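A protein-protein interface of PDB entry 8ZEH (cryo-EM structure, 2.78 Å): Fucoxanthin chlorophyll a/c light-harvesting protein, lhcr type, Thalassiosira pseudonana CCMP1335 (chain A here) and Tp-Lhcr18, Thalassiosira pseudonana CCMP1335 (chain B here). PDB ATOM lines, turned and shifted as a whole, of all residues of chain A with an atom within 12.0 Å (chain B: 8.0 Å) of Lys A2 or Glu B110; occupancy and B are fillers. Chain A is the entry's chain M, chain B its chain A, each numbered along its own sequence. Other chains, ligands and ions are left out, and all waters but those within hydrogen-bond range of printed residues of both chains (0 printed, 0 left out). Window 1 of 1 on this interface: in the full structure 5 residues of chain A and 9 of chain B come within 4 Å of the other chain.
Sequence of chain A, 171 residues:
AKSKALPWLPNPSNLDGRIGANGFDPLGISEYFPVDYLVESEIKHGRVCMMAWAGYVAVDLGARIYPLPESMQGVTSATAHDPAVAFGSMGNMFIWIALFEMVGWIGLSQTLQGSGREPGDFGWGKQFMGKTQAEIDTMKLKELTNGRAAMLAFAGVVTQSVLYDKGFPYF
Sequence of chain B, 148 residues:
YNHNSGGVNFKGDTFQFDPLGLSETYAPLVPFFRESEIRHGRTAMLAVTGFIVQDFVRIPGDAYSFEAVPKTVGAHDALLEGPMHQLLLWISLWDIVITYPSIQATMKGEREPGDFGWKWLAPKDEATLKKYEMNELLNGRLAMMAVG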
ATOM      1  N   ALA A   1      -1.018 -20.839 -17.338  1.00  0.00           N
ATOM      2  CA  ALA A   1      -1.958 -21.200 -16.287  1.00  0.00           C
ATOM      3  C   ALA A   1      -1.576 -20.546 -14.972  1.00  0.00           C
ATOM      4  O   ALA A   1      -0.532 -20.855 -14.401  1.00  0.00           O
ATOM      5  CB  ALA A   1      -2.017 -22.707 -16.131  1.00  0.00           C
ATOM      6  N   LYS A   2      -2.417 -19.642 -14.488  1.00  0.00           N
ATOM      7  CA  LYS A   2      -2.118 -18.935 -13.252  1.00  0.00           C
ATOM      8  C   LYS A   2      -2.575 -19.716 -12.031  1.00  0.00           C
ATOM      9  O   LYS A   2      -3.525 -20.491 -12.107  1.00  0.00           O
ATOM     10  CB  LYS A   2      -2.768 -17.557 -13.278  1.00  0.00           C
ATOM     11  CG  LYS A   2      -2.215 -16.648 -14.360  1.00  0.00           C
ATOM     12  CD  LYS A   2      -0.712 -16.488 -14.212  1.00  0.00           C
ATOM     13  CE  LYS A   2      -0.143 -15.584 -15.292  1.00  0.00           C
ATOM     14  NZ  LYS A   2      -0.432 -16.113 -16.652  1.00  0.00           N
ATOM     15  N   SER A   3      -1.901 -19.517 -10.904  1.00  0.00           N
ATOM     16  CA  SER A   3      -2.254 -20.233  -9.687  1.00  0.00           C
ATOM     17  C   SER A   3      -3.505 -19.662  -9.052  1.00  0.00           C
ATOM     18  O   SER A   3      -3.768 -18.468  -9.157  1.00  0.00           O
ATOM     19  CB  SER A   3      -1.106 -20.170  -8.689  1.00  0.00           C
ATOM     20  OG  SER A   3      -0.843 -18.837  -8.296  1.00  0.00           O
ATOM     21  N   LYS A   4      -4.274 -20.510  -8.385  1.00  0.00           N
ATOM     22  CA  LYS A   4      -5.492 -20.054  -7.732  1.00  0.00           C
ATOM     23  C   LYS A   4      -5.204 -19.083  -6.599  1.00  0.00           C
ATOM     24  O   LYS A   4      -5.862 -18.056  -6.482  1.00  0.00           O
ATOM     25  CB  LYS A   4      -6.279 -21.246  -7.195  1.00  0.00           C
ATOM     26  CG  LYS A   4      -7.578 -20.859  -6.517  1.00  0.00           C
ATOM     27  CD  LYS A   4      -8.372 -22.084  -6.105  1.00  0.00           C
ATOM     28  CE  LYS A   4      -9.735 -21.687  -5.566  1.00  0.00           C
ATOM     29  NZ  LYS A   4     -10.520 -20.920  -6.571  1.00  0.00           N
ATOM     30  N   ALA A   5      -4.228 -19.403  -5.762  1.00  0.00           N
ATOM     31  CA  ALA A   5      -3.912 -18.550  -4.623  1.00  0.00           C
ATOM     32  C   ALA A   5      -3.288 -17.241  -5.053  1.00  0.00           C
ATOM     33  O   ALA A   5      -3.642 -16.182  -4.536  1.00  0.00           O
ATOM     34  CB  ALA A   5      -2.983 -19.281  -3.676  1.00  0.00           C
ATOM     35  N   LEU A   6      -2.350 -17.309  -5.988  1.00  0.00           N
ATOM     36  CA  LEU A   6      -1.690 -16.108  -6.479  1.00  0.00           C
ATOM     37  C   LEU A   6      -2.031 -15.955  -7.942  1.00  0.00           C
ATOM     38  O   LEU A   6      -1.284 -16.402  -8.808  1.00  0.00           O
ATOM     39  CB  LEU A   6      -0.185 -16.207  -6.271  1.00  0.00           C
ATOM     40  CG  LEU A   6       0.243 -16.513  -4.834  1.00  0.00           C
ATOM     41  CD1 LEU A   6       1.758 -16.559  -4.714  1.00  0.00           C
ATOM     42  CD2 LEU A   6      -0.341 -15.494  -3.871  1.00  0.00           C
ATOM     43  N   PRO A   7      -3.160 -15.306  -8.234  1.00  0.00           N
ATOM     44  CA  PRO A   7      -3.614 -15.204  -9.626  1.00  0.00           C
ATOM     45  C   PRO A   7      -2.625 -14.560 -10.596  1.00  0.00           C
ATOM     46  O   PRO A   7      -2.716 -14.838 -11.787  1.00  0.00           O
ATOM     47  CB  PRO A   7      -4.867 -14.324  -9.513  1.00  0.00           C
ATOM     48  CG  PRO A   7      -4.785 -13.668  -8.175  1.00  0.00           C
ATOM     49  CD  PRO A   7      -4.085 -14.653  -7.298  1.00  0.00           C
ATOM     50  N   TRP A   8      -1.716 -13.719 -10.126  1.00  0.00           N
ATOM     51  CA  TRP A   8      -0.815 -13.014 -11.040  1.00  0.00           C
ATOM     52  C   TRP A   8       0.455 -13.791 -11.345  1.00  0.00           C
ATOM     53  O   TRP A   8       1.322 -13.301 -12.060  1.00  0.00           O
ATOM     54  CB  TRP A   8      -0.445 -11.641 -10.475  1.00  0.00           C
ATOM     55  CG  TRP A   8       0.295 -11.700  -9.188  1.00  0.00           C
ATOM     56  CD1 TRP A   8       1.637 -11.553  -9.009  1.00  0.00           C
ATOM     57  CD2 TRP A   8      -0.262 -11.924  -7.891  1.00  0.00           C
ATOM     58  NE1 TRP A   8       1.951 -11.671  -7.678  1.00  0.00           N
ATOM     59  CE2 TRP A   8       0.801 -11.899  -6.970  1.00  0.00           C
ATOM     60  CE3 TRP A   8      -1.558 -12.141  -7.418  1.00  0.00           C
ATOM     61  CZ2 TRP A   8       0.609 -12.084  -5.606  1.00  0.00           C
ATOM     62  CZ3 TRP A   8      -1.746 -12.324  -6.064  1.00  0.00           C
ATOM     63  CH2 TRP A   8      -0.669 -12.295  -5.174  1.00  0.00           C
ATOM     64  N   LEU A   9       0.571 -14.997 -10.808  1.00  0.00           N
ATOM     65  CA  LEU A   9       1.783 -15.781 -11.005  1.00  0.00           C
ATOM     66  C   LEU A   9       1.466 -17.140 -11.605  1.00  0.00           C
ATOM     67  O   LEU A   9       0.365 -17.657 -11.427  1.00  0.00           O
ATOM     68  CB  LEU A   9       2.525 -15.950  -9.680  1.00  0.00           C
ATOM     69  CG  LEU A   9       3.001 -14.661  -9.013  1.00  0.00           C
ATOM     70  CD1 LEU A   9       3.639 -14.957  -7.667  1.00  0.00           C
ATOM     71  CD2 LEU A   9       3.971 -13.925  -9.923  1.00  0.00           C
ATOM     72  N   PRO A  10       2.433 -17.730 -12.315  1.00  0.00           N
ATOM     73  CA  PRO A  10       2.221 -19.040 -12.934  1.00  0.00           C
ATOM     74  C   PRO A  10       1.963 -20.119 -11.897  1.00  0.00           C
ATOM     75  O   PRO A  10       2.356 -19.956 -10.746  1.00  0.00           O
ATOM     76  CB  PRO A  10       3.550 -19.308 -13.645  1.00  0.00           C
ATOM     77  CG  PRO A  10       4.543 -18.428 -12.965  1.00  0.00           C
ATOM     78  CD  PRO A  10       3.777 -17.199 -12.587  1.00  0.00           C
ATOM     79  N   ASN A  11       1.314 -21.207 -12.294  1.00  0.00           N
ATOM     80  CA  ASN A  11       0.979 -22.275 -11.357  1.00  0.00           C
ATOM     81  C   ASN A  11       2.110 -23.259 -11.141  1.00  0.00           C
ATOM     82  O   ASN A  11       2.755 -23.684 -12.096  1.00  0.00           O
ATOM     83  CB  ASN A  11      -0.239 -23.042 -11.870  1.00  0.00           C
ATOM     84  CG  ASN A  11      -0.588 -24.233 -11.002  1.00  0.00           C
ATOM     85  OD1 ASN A  11      -0.610 -24.137  -9.777  1.00  0.00           O
ATOM     86  ND2 ASN A  11      -0.880 -25.360 -11.636  1.00  0.00           N
ATOM     87  N   PRO A  12       2.367 -23.629  -9.878  1.00  0.00           N
ATOM     88  CA  PRO A  12       3.371 -24.670  -9.650  1.00  0.00           C
ATOM     89  C   PRO A  12       2.832 -25.985 -10.174  1.00  0.00           C
ATOM     90  O   PRO A  12       1.813 -26.450  -9.670  1.00  0.00           O
ATOM     91  CB  PRO A  12       3.501 -24.710  -8.128  1.00  0.00           C
ATOM     92  CG  PRO A  12       2.284 -24.024  -7.599  1.00  0.00           C
ATOM     93  CD  PRO A  12       1.917 -23.002  -8.627  1.00  0.00           C
ATOM     94  N   SER A  13       3.486 -26.583 -11.161  1.00  0.00           N
ATOM     95  CA  SER A  13       2.958 -27.800 -11.785  1.00  0.00           C
ATOM     96  C   SER A  13       3.238 -29.099 -11.045  1.00  0.00           C
ATOM     97  O   SER A  13       2.358 -29.947 -10.937  1.00  0.00           O
ATOM     98  CB  SER A  13       3.517 -27.924 -13.200  1.00  0.00           C
ATOM     99  OG  SER A  13       4.927 -28.049 -13.174  1.00  0.00           O
ATOM    100  N   ASN A  14       4.450 -29.272 -10.539  1.00  0.00           N
ATOM    101  CA  ASN A  14       4.810 -30.535  -9.897  1.00  0.00           C
ATOM    102  C   ASN A  14       3.933 -30.851  -8.695  1.00  0.00           C
ATOM    103  O   ASN A  14       3.831 -32.005  -8.289  1.00  0.00           O
ATOM    104  CB  ASN A  14       6.276 -30.505  -9.477  1.00  0.00           C
ATOM    105  CG  ASN A  14       7.196 -30.085 -10.604  1.00  0.00           C
ATOM    106  OD1 ASN A  14       6.773 -29.958 -11.752  1.00  0.00           O
ATOM    107  ND2 ASN A  14       8.465 -29.867 -10.281  1.00  0.00           N
ATOM    108  N   LEU A  15       3.300 -29.834  -8.121  1.00  0.00           N
ATOM    109  CA  LEU A  15       2.465 -30.038  -6.945  1.00  0.00           C
ATOM    110  C   LEU A  15       1.044 -30.405  -7.322  1.00  0.00           C
ATOM    111  O   LEU A  15       0.218 -30.670  -6.453  1.00  0.00           O
ATOM    112  CB  LEU A  15       2.450 -28.777  -6.086  1.00  0.00           C
ATOM    113  CG  LEU A  15       3.800 -28.298  -5.563  1.00  0.00           C
ATOM    114  CD1 LEU A  15       3.671 -26.909  -4.959  1.00  0.00           C
ATOM    115  CD2 LEU A  15       4.362 -29.286  -4.552  1.00  0.00           C
ATOM    116  N   ASP A  16       0.750 -30.423  -8.613  1.00  0.00           N
ATOM    117  CA  ASP A  16      -0.604 -30.714  -9.061  1.00  0.00           C
ATOM    118  C   ASP A  16      -1.026 -32.117  -8.675  1.00  0.00           C
ATOM    119  O   ASP A  16      -0.201 -33.022  -8.613  1.00  0.00           O
ATOM    120  CB  ASP A  16      -0.711 -30.539 -10.575  1.00  0.00           C
ATOM    121  CG  ASP A  16      -0.488 -29.105 -11.012  1.00  0.00           C
ATOM    122  OD1 ASP A  16      -0.475 -28.851 -12.234  1.00  0.00           O
ATOM    123  OD2 ASP A  16      -0.325 -28.233 -10.135  1.00  0.00           O
ATOM    124  N   ALA A  21      -3.278 -28.860  -2.424  1.00  0.00           N
ATOM    125  CA  ALA A  21      -2.631 -28.027  -3.426  1.00  0.00           C
ATOM    126  C   ALA A  21      -3.503 -26.838  -3.769  1.00  0.00           C
ATOM    127  O   ALA A  21      -4.428 -26.955  -4.567  1.00  0.00           O
ATOM    128  CB  ALA A  21      -2.336 -28.836  -4.671  1.00  0.00           C
ATOM    129  N   ASN A  22      -3.216 -25.690  -3.169  1.00  0.00           N
ATOM    130  CA  ASN A  22      -3.997 -24.493  -3.431  1.00  0.00           C
ATOM    131  C   ASN A  22      -3.262 -23.590  -4.399  1.00  0.00           C
ATOM    132  O   ASN A  22      -3.653 -22.445  -4.603  1.00  0.00           O
ATOM    133  CB  ASN A  22      -4.281 -23.754  -2.128  1.00  0.00           C
ATOM    134  CG  ASN A  22      -5.086 -24.586  -1.153  1.00  0.00           C
ATOM    135  OD1 ASN A  22      -5.474 -25.712  -1.455  1.00  0.00           O
ATOM    136  ND2 ASN A  22      -5.341 -24.032   0.025  1.00  0.00           N
ATOM    137  N   GLY A  23      -2.192 -24.100  -4.996  1.00  0.00           N
ATOM    138  CA  GLY A  23      -1.415 -23.313  -5.937  1.00  0.00           C
ATOM    139  C   GLY A  23      -0.474 -22.326  -5.282  1.00  0.00           C
ATOM    140  O   GLY A  23      -0.054 -21.364  -5.916  1.00  0.00           O
ATOM    141  N   PHE A  24      -0.137 -22.552  -4.018  1.00  0.00           N
ATOM    142  CA  PHE A  24       0.715 -21.609  -3.301  1.00  0.00           C
ATOM    143  C   PHE A  24       2.153 -22.073  -3.164  1.00  0.00           C
ATOM    144  O   PHE A  24       2.469 -22.851  -2.270  1.00  0.00           O
ATOM    145  CB  PHE A  24       0.144 -21.319  -1.913  1.00  0.00           C
ATOM    146  CG  PHE A  24       0.935 -20.312  -1.132  1.00  0.00           C
ATOM    147  CD1 PHE A  24       0.879 -18.970  -1.456  1.00  0.00           C
ATOM    148  CD2 PHE A  24       1.731 -20.707  -0.070  1.00  0.00           C
ATOM    149  CE1 PHE A  24       1.605 -18.039  -0.741  1.00  0.00           C
ATOM    150  CE2 PHE A  24       2.458 -19.781   0.651  1.00  0.00           C
ATOM    151  CZ  PHE A  24       2.395 -18.445   0.314  1.00  0.00           C
ATOM    152  N   ASP A  25       3.025 -21.610  -4.047  1.00  0.00           N
ATOM    153  CA  ASP A  25       4.440 -21.925  -3.942  1.00  0.00           C
ATOM    154  C   ASP A  25       5.153 -20.773  -4.600  1.00  0.00           C
ATOM    155  O   ASP A  25       5.799 -20.944  -5.631  1.00  0.00           O
ATOM    156  CB  ASP A  25       4.787 -23.236  -4.629  1.00  0.00           C
ATOM    157  CG  ASP A  25       6.240 -23.624  -4.440  1.00  0.00           C
ATOM    158  OD1 ASP A  25       6.936 -22.963  -3.642  1.00  0.00           O
ATOM    159  OD2 ASP A  25       6.688 -24.593  -5.087  1.00  0.00           O
ATOM    160  N   PRO A  26       5.043 -19.579  -4.010  1.00  0.00           N
ATOM    161  CA  PRO A  26       5.624 -18.402  -4.658  1.00  0.00           C
ATOM    162  C   PRO A  26       7.109 -18.544  -4.975  1.00  0.00           C
ATOM    163  O   PRO A  26       7.523 -18.145  -6.058  1.00  0.00           O
ATOM    164  CB  PRO A  26       5.416 -17.298  -3.615  1.00  0.00           C
ATOM    165  CG  PRO A  26       5.140 -18.001  -2.329  1.00  0.00           C
ATOM    166  CD  PRO A  26       4.426 -19.253  -2.717  1.00  0.00           C
ATOM    167  N   GLU A  31       9.700 -26.767  -7.693  1.00  0.00           N
ATOM    168  CA  GLU A  31      10.331 -26.915  -8.995  1.00  0.00           C
ATOM    169  C   GLU A  31      11.731 -27.477  -8.866  1.00  0.00           C
ATOM    170  O   GLU A  31      12.257 -28.049  -9.815  1.00  0.00           O
ATOM    171  CB  GLU A  31      10.371 -25.570  -9.715  1.00  0.00           C
ATOM    172  CG  GLU A  31       9.067 -24.793  -9.628  1.00  0.00           C
ATOM    173  CD  GLU A  31       7.888 -25.551 -10.208  1.00  0.00           C
ATOM    174  OE1 GLU A  31       8.099 -26.404 -11.097  1.00  0.00           O
ATOM    175  OE2 GLU A  31       6.745 -25.286  -9.783  1.00  0.00           O
ATOM    176  N   SER B 102       7.488 -12.339  -8.807  1.00  0.00           N
ATOM    177  CA  SER B 102       6.776 -11.620  -9.848  1.00  0.00           C
ATOM    178  C   SER B 102       7.724 -11.109 -10.919  1.00  0.00           C
ATOM    179  O   SER B 102       7.435 -11.216 -12.107  1.00  0.00           O
ATOM    180  CB  SER B 102       6.005 -10.458  -9.239  1.00  0.00           C
ATOM    181  OG  SER B 102       5.114 -10.913  -8.237  1.00  0.00           O
ATOM    182  N   ILE B 103       8.858 -10.556 -10.507  1.00  0.00           N
ATOM    183  CA  ILE B 103       9.812 -10.025 -11.468  1.00  0.00           C
ATOM    184  C   ILE B 103      10.279 -11.134 -12.389  1.00  0.00           C
ATOM    185  O   ILE B 103      10.382 -10.947 -13.594  1.00  0.00           O
ATOM    186  CB  ILE B 103      11.032  -9.392 -10.779  1.00  0.00           C
ATOM    187  CG1 ILE B 103      10.605  -8.191  -9.938  1.00  0.00           C
ATOM    188  CG2 ILE B 103      12.069  -8.972 -11.807  1.00  0.00           C
ATOM    189  CD1 ILE B 103      11.743  -7.545  -9.182  1.00  0.00           C
ATOM    190  N   GLN B 104      10.540 -12.305 -11.824  1.00  0.00           N
ATOM    191  CA  GLN B 104      11.008 -13.422 -12.630  1.00  0.00           C
ATOM    192  C   GLN B 104       9.992 -13.747 -13.707  1.00  0.00           C
ATOM    193  O   GLN B 104      10.357 -14.043 -14.841  1.00  0.00           O
ATOM    194  CB  GLN B 104      11.282 -14.643 -11.754  1.00  0.00           C
ATOM    195  CG  GLN B 104      12.283 -14.378 -10.643  1.00  0.00           C
ATOM    196  CD  GLN B 104      13.607 -13.854 -11.164  1.00  0.00           C
ATOM    197  OE1 GLN B 104      13.977 -14.095 -12.314  1.00  0.00           O
ATOM    198  NE2 GLN B 104      14.333 -13.137 -10.316  1.00  0.00           N
ATOM    199  N   ALA B 105       8.715 -13.684 -13.362  1.00  0.00           N
ATOM    200  CA  ALA B 105       7.676 -13.933 -14.349  1.00  0.00           C
ATOM    201  C   ALA B 105       7.695 -12.884 -15.449  1.00  0.00           C
ATOM    202  O   ALA B 105       7.625 -13.218 -16.628  1.00  0.00           O
ATOM    203  CB  ALA B 105       6.314 -13.972 -13.684  1.00  0.00           C
ATOM    204  N   THR B 106       7.795 -11.614 -15.072  1.00  0.00           N
ATOM    205  CA  THR B 106       7.759 -10.546 -16.066  1.00  0.00           C
ATOM    206  C   THR B 106       8.977 -10.619 -16.965  1.00  0.00           C
ATOM    207  O   THR B 106       8.933 -10.186 -18.111  1.00  0.00           O
ATOM    208  CB  THR B 106       7.665  -9.149 -15.421  1.00  0.00           C
ATOM    209  OG1 THR B 106       7.227  -8.200 -16.402  1.00  0.00           O
ATOM    210  CG2 THR B 106       9.007  -8.708 -14.871  1.00  0.00           C
ATOM    211  N   MET B 107      10.064 -11.177 -16.452  1.00  0.00           N
ATOM    212  CA  MET B 107      11.279 -11.309 -17.246  1.00  0.00           C
ATOM    213  C   MET B 107      11.171 -12.466 -18.230  1.00  0.00           C
ATOM    214  O   MET B 107      12.089 -12.707 -19.010  1.00  0.00           O
ATOM    215  CB  MET B 107      12.496 -11.507 -16.343  1.00  0.00           C
ATOM    216  CG  MET B 107      12.781 -10.341 -15.412  1.00  0.00           C
ATOM    217  SD  MET B 107      13.225  -8.831 -16.288  1.00  0.00           S
ATOM    218  CE  MET B 107      14.766  -9.322 -17.055  1.00  0.00           C
ATOM    219  N   LYS B 108      10.071 -13.204 -18.171  1.00  0.00           N
ATOM    220  CA  LYS B 108       9.880 -14.314 -19.089  1.00  0.00           C
ATOM    221  C   LYS B 108       8.632 -14.096 -19.924  1.00  0.00           C
ATOM    222  O   LYS B 108       8.282 -14.936 -20.750  1.00  0.00           O
ATOM    223  CB  LYS B 108       9.788 -15.636 -18.331  1.00  0.00           C
ATOM    224  CG  LYS B 108      10.955 -15.904 -17.399  1.00  0.00           C
ATOM    225  CD  LYS B 108      10.861 -17.300 -16.810  1.00  0.00           C
ATOM    226  CE  LYS B 108       9.534 -17.509 -16.100  1.00  0.00           C
ATOM    227  NZ  LYS B 108       9.393 -16.621 -14.915  1.00  0.00           N
ATOM    228  N   GLY B 109       7.957 -12.972 -19.712  1.00  0.00           N
ATOM    229  CA  GLY B 109       6.779 -12.657 -20.501  1.00  0.00           C
ATOM    230  C   GLY B 109       5.477 -13.274 -20.038  1.00  0.00           C
ATOM    231  O   GLY B 109       4.636 -13.627 -20.861  1.00  0.00           O
ATOM    232  N   GLU B 110       5.296 -13.408 -18.730  1.00  0.00           N
ATOM    233  CA  GLU B 110       4.037 -13.932 -18.214  1.00  0.00           C
ATOM    234  C   GLU B 110       3.302 -12.926 -17.342  1.00  0.00           C
ATOM    235  O   GLU B 110       2.164 -13.161 -16.948  1.00  0.00           O
ATOM    236  CB  GLU B 110       4.267 -15.221 -17.426  1.00  0.00           C
ATOM    237  CG  GLU B 110       4.743 -16.391 -18.269  1.00  0.00           C
ATOM    238  CD  GLU B 110       6.204 -16.271 -18.639  1.00  0.00           C
ATOM    239  OE1 GLU B 110       6.899 -15.451 -18.009  1.00  0.00           O
ATOM    240  OE2 GLU B 110       6.655 -16.994 -19.550  1.00  0.00           O
ATOM    241  N   ARG B 111       3.949 -11.810 -17.032  1.00  0.00           N
ATOM    242  CA  ARG B 111       3.310 -10.789 -16.218  1.00  0.00           C
ATOM    243  C   ARG B 111       3.583  -9.411 -16.768  1.00  0.00           C
ATOM    244  O   ARG B 111       4.710  -9.104 -17.147  1.00  0.00           O
ATOM    245  CB  ARG B 111       3.795 -10.865 -14.772  1.00  0.00           C
ATOM    246  CG  ARG B 111       3.016  -9.979 -13.815  1.00  0.00           C
ATOM    247  CD  ARG B 111       3.555 -10.085 -12.400  1.00  0.00           C
ATOM    248  NE  ARG B 111       4.900  -9.534 -12.292  1.00  0.00           N
ATOM    249  CZ  ARG B 111       5.164  -8.270 -11.982  1.00  0.00           C
ATOM    250  NH1 ARG B 111       4.172  -7.424 -11.746  1.00  0.00           N
ATOM    251  NH2 ARG B 111       6.419  -7.853 -11.907  1.00  0.00           N
ATOM    252  N   GLU B 112       2.557  -8.573 -16.821  1.00  0.00           N
ATOM    253  CA  GLU B 112       2.756  -7.209 -17.266  1.00  0.00           C
ATOM    254  C   GLU B 112       3.326  -6.419 -16.112  1.00  0.00           C
ATOM    255  O   GLU B 112       2.854  -6.535 -14.985  1.00  0.00           O
ATOM    256  CB  GLU B 112       1.441  -6.596 -17.725  1.00  0.00           C
ATOM    257  CG  GLU B 112       0.760  -7.367 -18.842  1.00  0.00           C
ATOM    258  CD  GLU B 112       1.562  -7.364 -20.129  1.00  0.00           C
ATOM    259  OE1 GLU B 112       2.516  -6.565 -20.241  1.00  0.00           O
ATOM    260  OE2 GLU B 112       1.231  -8.157 -21.036  1.00  0.00           O
ATOM    261  N   PRO B 113       4.356  -5.613 -16.380  1.00  0.00           N
ATOM    262  CA  PRO B 113       4.997  -4.886 -15.286  1.00  0.00           C
ATOM    263  C   PRO B 113       3.985  -4.110 -14.462  1.00  0.00           C
ATOM    264  O   PRO B 113       3.189  -3.366 -15.026  1.00  0.00           O
ATOM    265  CB  PRO B 113       5.922  -3.921 -16.019  1.00  0.00           C
ATOM    266  CG  PRO B 113       6.266  -4.631 -17.283  1.00  0.00           C
ATOM    267  CD  PRO B 113       5.033  -5.398 -17.669  1.00  0.00           C
ATOM    268  N   ASP B 115       1.657  -5.488 -12.400  1.00  0.00           N
ATOM    269  CA  ASP B 115       0.485  -6.270 -12.029  1.00  0.00           C
ATOM    270  C   ASP B 115       0.727  -7.097 -10.785  1.00  0.00           C
ATOM    271  O   ASP B 115       1.711  -7.831 -10.704  1.00  0.00           O
ATOM    272  CB  ASP B 115       0.069  -7.193 -13.173  1.00  0.00           C
ATOM    273  CG  ASP B 115      -1.189  -7.976 -12.859  1.00  0.00           C
ATOM    274  OD1 ASP B 115      -1.909  -7.597 -11.910  1.00  0.00           O
ATOM    275  OD2 ASP B 115      -1.463  -8.966 -13.567  1.00  0.00           O
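The indole nitrogen (NE1) of Trp A8 lies within hydrogen-bond range of the side-chain hydroxyl (OG) of Ser B102, 3.3 Å away.
Ala A1 touches none of the printed residues of chain B. Ala A5 touches none of the printed residues of chain B. Of the printed residues of chain A, Ser B102 touches Trp A8 and Leu A9. No residue of chain A comes within 4 Å of Thr B106. No residue of chain A comes within 4 Å of Lys B108. Glu B110 touches just one residue of chain A: Lys A2 (3.7 Å). Printed residues of chain A within 4 Å of Arg B111: Trp A8. No residue of chain A comes within 4 Å of Glu B112.
Printed residues of chain B that touch a printed residue of chain A: Ser B102, Glu B110 and Arg B111. Of the 23 printed residues of chain A, 3 touch a printed residue of chain B.
The backbone carbonyl oxygen of Arg B111 sits at hydrogen-bond distance from the side-chain hydroxyl of Thr B106, 2.8 Å away. The backbone carbonyl oxygen of Ser B102 lies within hydrogen-bond range of the guanidinium group of Arg B111, 3.0 Å away. The backbone NH (N) of Ser A3 lies within hydrogen-bond range of the backbone carbonyl oxygen (O) of Leu A9 (3.0 Å). O of Ala B105 lies within hydrogen-bond range of N of Glu B110 (3.1 Å). The backbone carbonyl oxygen (O) of Asp B115 is in hydrogen-bond range of the guanidinium group (NH1) of Arg B111 (2.7 Å).
O of Glu B110 touches CE of Lys A2, 3.7 Å away. Arg B111 touches Trp A8. Leu A9 touches Ser B102.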
